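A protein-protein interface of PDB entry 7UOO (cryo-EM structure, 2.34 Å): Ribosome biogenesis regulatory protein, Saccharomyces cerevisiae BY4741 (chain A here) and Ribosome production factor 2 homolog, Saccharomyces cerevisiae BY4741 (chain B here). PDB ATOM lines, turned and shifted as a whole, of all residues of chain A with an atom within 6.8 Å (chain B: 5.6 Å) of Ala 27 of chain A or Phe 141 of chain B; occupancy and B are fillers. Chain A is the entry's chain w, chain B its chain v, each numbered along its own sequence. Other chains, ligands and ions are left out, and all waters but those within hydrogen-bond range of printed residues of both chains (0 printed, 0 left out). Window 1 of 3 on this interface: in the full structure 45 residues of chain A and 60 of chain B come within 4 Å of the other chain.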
ATOM      1  N   VAL A  20       1.977   9.659  31.032  1.00  0.00           N
ATOM      2  CA  VAL A  20       2.340  11.057  31.205  1.00  0.00           C
ATOM      3  C   VAL A  20       2.819  11.602  29.867  1.00  0.00           C
ATOM      4  O   VAL A  20       3.229  10.860  28.972  1.00  0.00           O
ATOM      5  CB  VAL A  20       3.410  11.258  32.299  1.00  0.00           C
ATOM      6  CG1 VAL A  20       2.962  10.619  33.602  1.00  0.00           C
ATOM      7  CG2 VAL A  20       4.751  10.697  31.858  1.00  0.00           C
ATOM      8  N   TYR A  21       2.747  12.923  29.735  1.00  0.00           N
ATOM      9  CA  TYR A  21       3.062  13.596  28.486  1.00  0.00           C
ATOM     10  C   TYR A  21       4.056  14.720  28.725  1.00  0.00           C
ATOM     11  O   TYR A  21       4.027  15.392  29.759  1.00  0.00           O
ATOM     12  CB  TYR A  21       1.805  14.177  27.822  1.00  0.00           C
ATOM     13  CG  TYR A  21       0.687  13.187  27.612  1.00  0.00           C
ATOM     14  CD1 TYR A  21       0.719  12.288  26.557  1.00  0.00           C
ATOM     15  CD2 TYR A  21      -0.412  13.164  28.461  1.00  0.00           C
ATOM     16  CE1 TYR A  21      -0.305  11.386  26.356  1.00  0.00           C
ATOM     17  CE2 TYR A  21      -1.443  12.266  28.270  1.00  0.00           C
ATOM     18  CZ  TYR A  21      -1.384  11.379  27.216  1.00  0.00           C
ATOM     19  OH  TYR A  21      -2.407  10.480  27.019  1.00  0.00           O
ATOM     20  N   ASP A  22       4.937  14.919  27.747  1.00  0.00           N
ATOM     21  CA  ASP A  22       5.778  16.108  27.638  1.00  0.00           C
ATOM     22  C   ASP A  22       5.531  16.622  26.225  1.00  0.00           C
ATOM     23  O   ASP A  22       6.224  16.233  25.282  1.00  0.00           O
ATOM     24  CB  ASP A  22       7.246  15.793  27.894  1.00  0.00           C
ATOM     25  CG  ASP A  22       8.099  17.040  28.002  1.00  0.00           C
ATOM     26  OD1 ASP A  22       7.528  18.145  28.098  1.00  0.00           O
ATOM     27  OD2 ASP A  22       9.340  16.916  27.989  1.00  0.00           O
ATOM     28  N   LEU A  23       4.509  17.469  26.076  1.00  0.00           N
ATOM     29  CA  LEU A  23       4.119  17.942  24.753  1.00  0.00           C
ATOM     30  C   LEU A  23       5.127  18.922  24.166  1.00  0.00           C
ATOM     31  O   LEU A  23       5.146  19.111  22.945  1.00  0.00           O
ATOM     32  CB  LEU A  23       2.734  18.582  24.814  1.00  0.00           C
ATOM     33  CG  LEU A  23       1.617  17.663  25.315  1.00  0.00           C
ATOM     34  CD1 LEU A  23       0.275  18.373  25.298  1.00  0.00           C
ATOM     35  CD2 LEU A  23       1.561  16.388  24.492  1.00  0.00           C
ATOM     36  N   GLY A  24       5.958  19.546  25.002  1.00  0.00           N
ATOM     37  CA  GLY A  24       7.026  20.379  24.478  1.00  0.00           C
ATOM     38  C   GLY A  24       8.072  19.576  23.731  1.00  0.00           C
ATOM     39  O   GLY A  24       8.594  20.020  22.706  1.00  0.00           O
ATOM     40  N   ASN A  25       8.398  18.388  24.235  1.00  0.00           N
ATOM     41  CA  ASN A  25       9.296  17.465  23.557  1.00  0.00           C
ATOM     42  C   ASN A  25       8.560  16.496  22.642  1.00  0.00           C
ATOM     43  O   ASN A  25       9.210  15.652  22.015  1.00  0.00           O
ATOM     44  CB  ASN A  25      10.115  16.669  24.579  1.00  0.00           C
ATOM     45  CG  ASN A  25      11.042  17.544  25.395  1.00  0.00           C
ATOM     46  OD1 ASN A  25      11.494  18.591  24.932  1.00  0.00           O
ATOM     47  ND2 ASN A  25      11.337  17.116  26.616  1.00  0.00           N
ATOM     48  N   LEU A  26       7.229  16.605  22.553  1.00  0.00           N
ATOM     49  CA  LEU A  26       6.388  15.694  21.770  1.00  0.00           C
ATOM     50  C   LEU A  26       6.603  14.237  22.178  1.00  0.00           C
ATOM     51  O   LEU A  26       6.729  13.351  21.332  1.00  0.00           O
ATOM     52  CB  LEU A  26       6.619  15.871  20.266  1.00  0.00           C
ATOM     53  CG  LEU A  26       6.349  17.241  19.648  1.00  0.00           C
ATOM     54  CD1 LEU A  26       6.651  17.223  18.160  1.00  0.00           C
ATOM     55  CD2 LEU A  26       4.917  17.669  19.896  1.00  0.00           C
ATOM     56  N   ALA A  27       6.645  13.985  23.484  1.00  0.00           N
ATOM     57  CA  ALA A  27       6.926  12.659  24.014  1.00  0.00           C
ATOM     58  C   ALA A  27       5.795  12.187  24.919  1.00  0.00           C
ATOM     59  O   ALA A  27       5.159  12.982  25.617  1.00  0.00           O
ATOM     60  CB  ALA A  27       8.245  12.644  24.792  1.00  0.00           C
ATOM     61  N   ALA A  28       5.545  10.881  24.892  1.00  0.00           N
ATOM     62  CA  ALA A  28       4.579  10.244  25.776  1.00  0.00           C
ATOM     63  C   ALA A  28       5.254   9.071  26.467  1.00  0.00           C
ATOM     64  O   ALA A  28       5.900   8.250  25.808  1.00  0.00           O
ATOM     65  CB  ALA A  28       3.342   9.770  25.006  1.00  0.00           C
ATOM     66  N   PHE A  29       5.110   8.993  27.788  1.00  0.00           N
ATOM     67  CA  PHE A  29       5.738   7.946  28.586  1.00  0.00           C
ATOM     68  C   PHE A  29       4.660   7.121  29.270  1.00  0.00           C
ATOM     69  O   PHE A  29       3.843   7.663  30.024  1.00  0.00           O
ATOM     70  CB  PHE A  29       6.690   8.539  29.627  1.00  0.00           C
ATOM     71  CG  PHE A  29       7.620   9.579  29.078  1.00  0.00           C
ATOM     72  CD1 PHE A  29       8.749   9.213  28.369  1.00  0.00           C
ATOM     73  CD2 PHE A  29       7.374  10.926  29.286  1.00  0.00           C
ATOM     74  CE1 PHE A  29       9.610  10.169  27.866  1.00  0.00           C
ATOM     75  CE2 PHE A  29       8.231  11.886  28.786  1.00  0.00           C
ATOM     76  CZ  PHE A  29       9.350  11.507  28.076  1.00  0.00           C
ATOM     77  N   ASN A  57       0.117   4.364  22.221  1.00  0.00           N
ATOM     78  CA  ASN A  57       0.763   5.542  22.796  1.00  0.00           C
ATOM     79  C   ASN A  57       0.731   6.723  21.828  1.00  0.00           C
ATOM     80  O   ASN A  57       0.500   7.868  22.239  1.00  0.00           O
ATOM     81  CB  ASN A  57       2.199   5.209  23.195  1.00  0.00           C
ATOM     82  CG  ASN A  57       2.278   4.041  24.153  1.00  0.00           C
ATOM     83  OD1 ASN A  57       3.176   3.208  24.058  1.00  0.00           O
ATOM     84  ND2 ASN A  57       1.326   3.968  25.077  1.00  0.00           N
ATOM     85  N   VAL A  58       0.953   6.461  20.538  1.00  0.00           N
ATOM     86  CA  VAL A  58       0.904   7.515  19.530  1.00  0.00           C
ATOM     87  C   VAL A  58      -0.508   8.074  19.410  1.00  0.00           C
ATOM     88  O   VAL A  58      -0.693   9.281  19.227  1.00  0.00           O
ATOM     89  CB  VAL A  58       1.433   6.982  18.186  1.00  0.00           C
ATOM     90  CG1 VAL A  58       1.032   7.887  17.034  1.00  0.00           C
ATOM     91  CG2 VAL A  58       2.939   6.861  18.235  1.00  0.00           C
ATOM     92  N   LEU A  61      -0.933  10.440  22.309  1.00  0.00           N
ATOM     93  CA  LEU A  61      -0.157  11.660  22.095  1.00  0.00           C
ATOM     94  C   LEU A  61      -0.809  12.557  21.048  1.00  0.00           C
ATOM     95  O   LEU A  61      -0.842  13.783  21.205  1.00  0.00           O
ATOM     96  CB  LEU A  61       1.270  11.304  21.685  1.00  0.00           C
ATOM     97  CG  LEU A  61       2.238  12.471  21.498  1.00  0.00           C
ATOM     98  CD1 LEU A  61       2.525  13.149  22.826  1.00  0.00           C
ATOM     99  CD2 LEU A  61       3.523  11.999  20.842  1.00  0.00           C
ATOM    100  N   THR A  97      10.511  17.731  30.612  1.00  0.00           N
ATOM    101  CA  THR A  97      11.703  16.935  30.873  1.00  0.00           C
ATOM    102  C   THR A  97      12.940  17.823  30.902  1.00  0.00           C
ATOM    103  O   THR A  97      13.123  18.681  30.035  1.00  0.00           O
ATOM    104  CB  THR A  97      11.858  15.852  29.807  1.00  0.00           C
ATOM    105  OG1 THR A  97      10.610  15.173  29.626  1.00  0.00           O
ATOM    106  CG2 THR A  97      12.918  14.844  30.214  1.00  0.00           C
ATOM    107  N   PRO B 139      10.821  14.537  15.454  1.00  0.00           N
ATOM    108  CA  PRO B 139       9.918  13.386  15.567  1.00  0.00           C
ATOM    109  C   PRO B 139       9.081  13.409  16.833  1.00  0.00           C
ATOM    110  O   PRO B 139       9.213  14.314  17.663  1.00  0.00           O
ATOM    111  CB  PRO B 139      10.886  12.202  15.580  1.00  0.00           C
ATOM    112  CG  PRO B 139      12.088  12.747  16.284  1.00  0.00           C
ATOM    113  CD  PRO B 139      12.184  14.211  15.911  1.00  0.00           C
ATOM    114  N   MET B 140       8.218  12.413  16.988  1.00  0.00           N
ATOM    115  CA  MET B 140       7.554  12.155  18.255  1.00  0.00           C
ATOM    116  C   MET B 140       8.282  11.031  18.977  1.00  0.00           C
ATOM    117  O   MET B 140       8.954  10.209  18.354  1.00  0.00           O
ATOM    118  CB  MET B 140       6.085  11.794  18.040  1.00  0.00           C
ATOM    119  CG  MET B 140       5.222  12.981  17.662  1.00  0.00           C
ATOM    120  SD  MET B 140       3.568  12.512  17.132  1.00  0.00           S
ATOM    121  CE  MET B 140       3.927  11.838  15.516  1.00  0.00           C
ATOM    122  N   PHE B 141       8.172  11.014  20.300  1.00  0.00           N
ATOM    123  CA  PHE B 141       8.883  10.046  21.124  1.00  0.00           C
ATOM    124  C   PHE B 141       7.897   9.204  21.917  1.00  0.00           C
ATOM    125  O   PHE B 141       6.867   9.705  22.378  1.00  0.00           O
ATOM    126  CB  PHE B 141       9.852  10.734  22.089  1.00  0.00           C
ATOM    127  CG  PHE B 141      11.036  11.363  21.419  1.00  0.00           C
ATOM    128  CD1 PHE B 141      10.980  12.672  20.972  1.00  0.00           C
ATOM    129  CD2 PHE B 141      12.208  10.649  21.245  1.00  0.00           C
ATOM    130  CE1 PHE B 141      12.068  13.254  20.358  1.00  0.00           C
ATOM    131  CE2 PHE B 141      13.301  11.226  20.633  1.00  0.00           C
ATOM    132  CZ  PHE B 141      13.232  12.531  20.189  1.00  0.00           C
ATOM    133  N   THR B 142       8.220   7.922  22.071  1.00  0.00           N
ATOM    134  CA  THR B 142       7.483   7.035  22.961  1.00  0.00           C
ATOM    135  C   THR B 142       8.479   6.179  23.728  1.00  0.00           C
ATOM    136  O   THR B 142       9.410   5.627  23.136  1.00  0.00           O
ATOM    137  CB  THR B 142       6.500   6.150  22.187  1.00  0.00           C
ATOM    138  OG1 THR B 142       7.110   5.707  20.970  1.00  0.00           O
ATOM    139  CG2 THR B 142       5.230   6.919  21.860  1.00  0.00           C
ATOM    140  N   PHE B 143       8.289   6.086  25.041  1.00  0.00           N
ATOM    141  CA  PHE B 143       9.159   5.308  25.912  1.00  0.00           C
ATOM    142  C   PHE B 143       8.312   4.345  26.728  1.00  0.00           C
ATOM    143  O   PHE B 143       7.382   4.768  27.422  1.00  0.00           O
ATOM    144  CB  PHE B 143       9.979   6.217  26.836  1.00  0.00           C
ATOM    145  CG  PHE B 143      11.136   6.888  26.154  1.00  0.00           C
ATOM    146  CD1 PHE B 143      10.946   8.036  25.404  1.00  0.00           C
ATOM    147  CD2 PHE B 143      12.414   6.367  26.262  1.00  0.00           C
ATOM    148  CE1 PHE B 143      12.011   8.652  24.776  1.00  0.00           C
ATOM    149  CE2 PHE B 143      13.480   6.978  25.635  1.00  0.00           C
ATOM    150  CZ  PHE B 143      13.278   8.123  24.892  1.00  0.00           C
ATOM    151  N   PHE B 161      18.620   9.859  24.645  1.00  0.00           N
ATOM    152  CA  PHE B 161      17.948   9.735  23.355  1.00  0.00           C
ATOM    153  C   PHE B 161      17.041  10.929  23.077  1.00  0.00           C
ATOM    154  O   PHE B 161      16.961  11.395  21.931  1.00  0.00           O
ATOM    155  CB  PHE B 161      17.172   8.422  23.286  1.00  0.00           C
ATOM    156  CG  PHE B 161      17.926   7.320  22.599  1.00  0.00           C
ATOM    157  CD1 PHE B 161      18.904   6.607  23.271  1.00  0.00           C
ATOM    158  CD2 PHE B 161      17.670   7.012  21.274  1.00  0.00           C
ATOM    159  CE1 PHE B 161      19.605   5.600  22.640  1.00  0.00           C
ATOM    160  CE2 PHE B 161      18.368   6.004  20.635  1.00  0.00           C
ATOM    161  CZ  PHE B 161      19.338   5.297  21.320  1.00  0.00           C
ATOM    162  N   LEU B 162      16.360  11.446  24.107  1.00  0.00           N
ATOM    163  CA  LEU B 162      15.568  12.659  23.924  1.00  0.00           C
ATOM    164  C   LEU B 162      16.448  13.831  23.510  1.00  0.00           C
ATOM    165  O   LEU B 162      16.113  14.565  22.574  1.00  0.00           O
ATOM    166  CB  LEU B 162      14.806  12.994  25.206  1.00  0.00           C
ATOM    167  CG  LEU B 162      13.437  12.346  25.412  1.00  0.00           C
ATOM    168  CD1 LEU B 162      12.941  12.589  26.828  1.00  0.00           C
ATOM    169  CD2 LEU B 162      12.436  12.877  24.399  1.00  0.00           C
ATOM    170  N   PHE B 165      17.808  13.133  19.696  1.00  0.00           N
ATOM    171  CA  PHE B 165      16.890  13.210  18.568  1.00  0.00           C
ATOM    172  C   PHE B 165      15.804  14.264  18.738  1.00  0.00           C
ATOM    173  O   PHE B 165      14.850  14.282  17.954  1.00  0.00           O
ATOM    174  CB  PHE B 165      16.253  11.842  18.312  1.00  0.00           C
ATOM    175  CG  PHE B 165      17.219  10.810  17.810  1.00  0.00           C
ATOM    176  CD1 PHE B 165      17.788  10.932  16.553  1.00  0.00           C
ATOM    177  CD2 PHE B 165      17.557   9.717  18.589  1.00  0.00           C
ATOM    178  CE1 PHE B 165      18.679   9.985  16.085  1.00  0.00           C
ATOM    179  CE2 PHE B 165      18.445   8.767  18.125  1.00  0.00           C
ATOM    180  CZ  PHE B 165      19.006   8.903  16.871  1.00  0.00           C
ATOM    181  N   ARG B 166      15.921  15.145  19.735  1.00  0.00           N
ATOM    182  CA  ARG B 166      14.903  16.173  19.923  1.00  0.00           C
ATOM    183  C   ARG B 166      14.937  17.199  18.796  1.00  0.00           C
ATOM    184  O   ARG B 166      13.895  17.554  18.236  1.00  0.00           O
ATOM    185  CB  ARG B 166      15.087  16.850  21.281  1.00  0.00           C
ATOM    186  CG  ARG B 166      14.028  17.885  21.585  1.00  0.00           C
ATOM    187  CD  ARG B 166      14.117  18.377  23.016  1.00  0.00           C
ATOM    188  NE  ARG B 166      15.412  18.970  23.323  1.00  0.00           N
ATOM    189  CZ  ARG B 166      15.642  19.754  24.366  1.00  0.00           C
ATOM    190  NH1 ARG B 166      14.678  20.080  25.211  1.00  0.00           N
ATOM    191  NH2 ARG B 166      16.868  20.227  24.563  1.00  0.00           N
ATOM    192  N   VAL B 181       7.562   8.615  14.440  1.00  0.00           N
ATOM    193  CA  VAL B 181       7.675   8.381  15.873  1.00  0.00           C
ATOM    194  C   VAL B 181       8.811   7.400  16.134  1.00  0.00           C
ATOM    195  O   VAL B 181       8.969   6.400  15.422  1.00  0.00           O
ATOM    196  CB  VAL B 181       6.344   7.871  16.471  1.00  0.00           C
ATOM    197  CG1 VAL B 181       5.813   6.681  15.687  1.00  0.00           C
ATOM    198  CG2 VAL B 181       6.506   7.523  17.946  1.00  0.00           C
ATOM    199  N   ILE B 182       9.619   7.712  17.143  1.00  0.00           N
ATOM    200  CA  ILE B 182      10.704   6.865  17.619  1.00  0.00           C
ATOM    201  C   ILE B 182      10.262   6.233  18.931  1.00  0.00           C
ATOM    202  O   ILE B 182       9.881   6.942  19.872  1.00  0.00           O
ATOM    203  CB  ILE B 182      11.995   7.677  17.809  1.00  0.00           C
ATOM    204  CG1 ILE B 182      12.532   8.151  16.457  1.00  0.00           C
ATOM    205  CG2 ILE B 182      13.026   6.871  18.573  1.00  0.00           C
ATOM    206  CD1 ILE B 182      13.713   9.080  16.567  1.00  0.00           C
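The backbone carbonyl oxygen of Leu 26 of chain A sits at hydrogen-bond distance from the backbone NH of Phe 141 of chain B (2.9 Å). The backbone NH of Phe 143 of chain B lies within hydrogen-bond range of the backbone carbonyl oxygen of Ala 28 of chain A (3.3 Å). The backbone carbonyl oxygen of Phe 141 of chain B is in hydrogen-bond range of the backbone NH of Ala 28 of chain A (3.1 Å).
N of Asp 22 of chain A is in hydrogen-bond range of O of Ala 27 of chain A, at 2.9 Å. The backbone carbonyl oxygen (O) of Met 140 of chain B is in hydrogen-bond range of the backbone NH (N) of Ile 182 of chain B, at 2.9 Å. The backbone carbonyl oxygen of Ile 182 of chain B lies within hydrogen-bond range of the backbone NH of Thr 142 of chain B (2.9 Å). The backbone NH (N) of Phe 29 of chain A sits at hydrogen-bond distance from the backbone carbonyl oxygen (O) of Val 20 of chain A (2.9 Å). The side-chain amide nitrogen (ND2) of Asn 25 of chain A lies within hydrogen-bond range of the side-chain carboxylate (OD2) of Asp 22 of chain A.
Among the printed residues, merely in contact across the chains: Asn 25 of chain A with Phe 141 of chain B, Asn 25 of chain A with Arg 166 of chain B, Leu 26 of chain A with Pro 139 of chain B, Leu 26 of chain A with Met 140 of chain B, Ala 27 of chain A with Phe 141 of chain B, Ala 28 of chain A with Thr 142 of chain B, Phe 29 of chain A with Phe 143 of chain B, Phe 29 of chain A with Leu 162 of chain B, Asn 57 of chain A with Thr 142 of chain B, Val 58 of chain A with Val 181 of chain B and Leu 61 of chain A with Met 140 of chain B.
Val 20 of chain A touches none of the printed residues of chain B. Printed residues of chain B within 4 Å of Asn 25 of chain A: Phe 141 and Arg 166. Of the printed residues of chain B, Leu 26 of chain A touches Pro 139, Met 140 and Phe 141. Of chain B, only Phe 141 comes within 4 Å of Ala 27 of chain A. Of the printed residues of chain B, Ala 28 of chain A touches Phe 141, Thr 142 and Phe 143. Of the printed residues of chain B, Val 58 of chain A touches Val 181 (3.6 Å). Thr 97 of chain A touches none of the printed residues of chain B. Of chain A, only Asn 25, Leu 26, Ala 27 and Ala 28 come within 4 Å of Phe 141 of chain B. The nearest residue of chain B that does not touch Ala 27 of chain A is Leu 162 of chain B (4.2 Å). The nearest residue of chain A that does not touch Phe 141 of chain B is Leu 61 of chain A (4.3 Å).
Of the 14 printed residues of chain A, 8 touch a printed residue of chain B. Hydrophobic or aromatic side chains of chain A within 4 Å of the printed part of chain B: Leu 26, Ala 27, Phe 29, Val 58 and Leu 61. Among the printed residues, no Asp or Glu carboxylate lies within 4 Å of a Lys or Arg side-chain nitrogen of the other chain.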
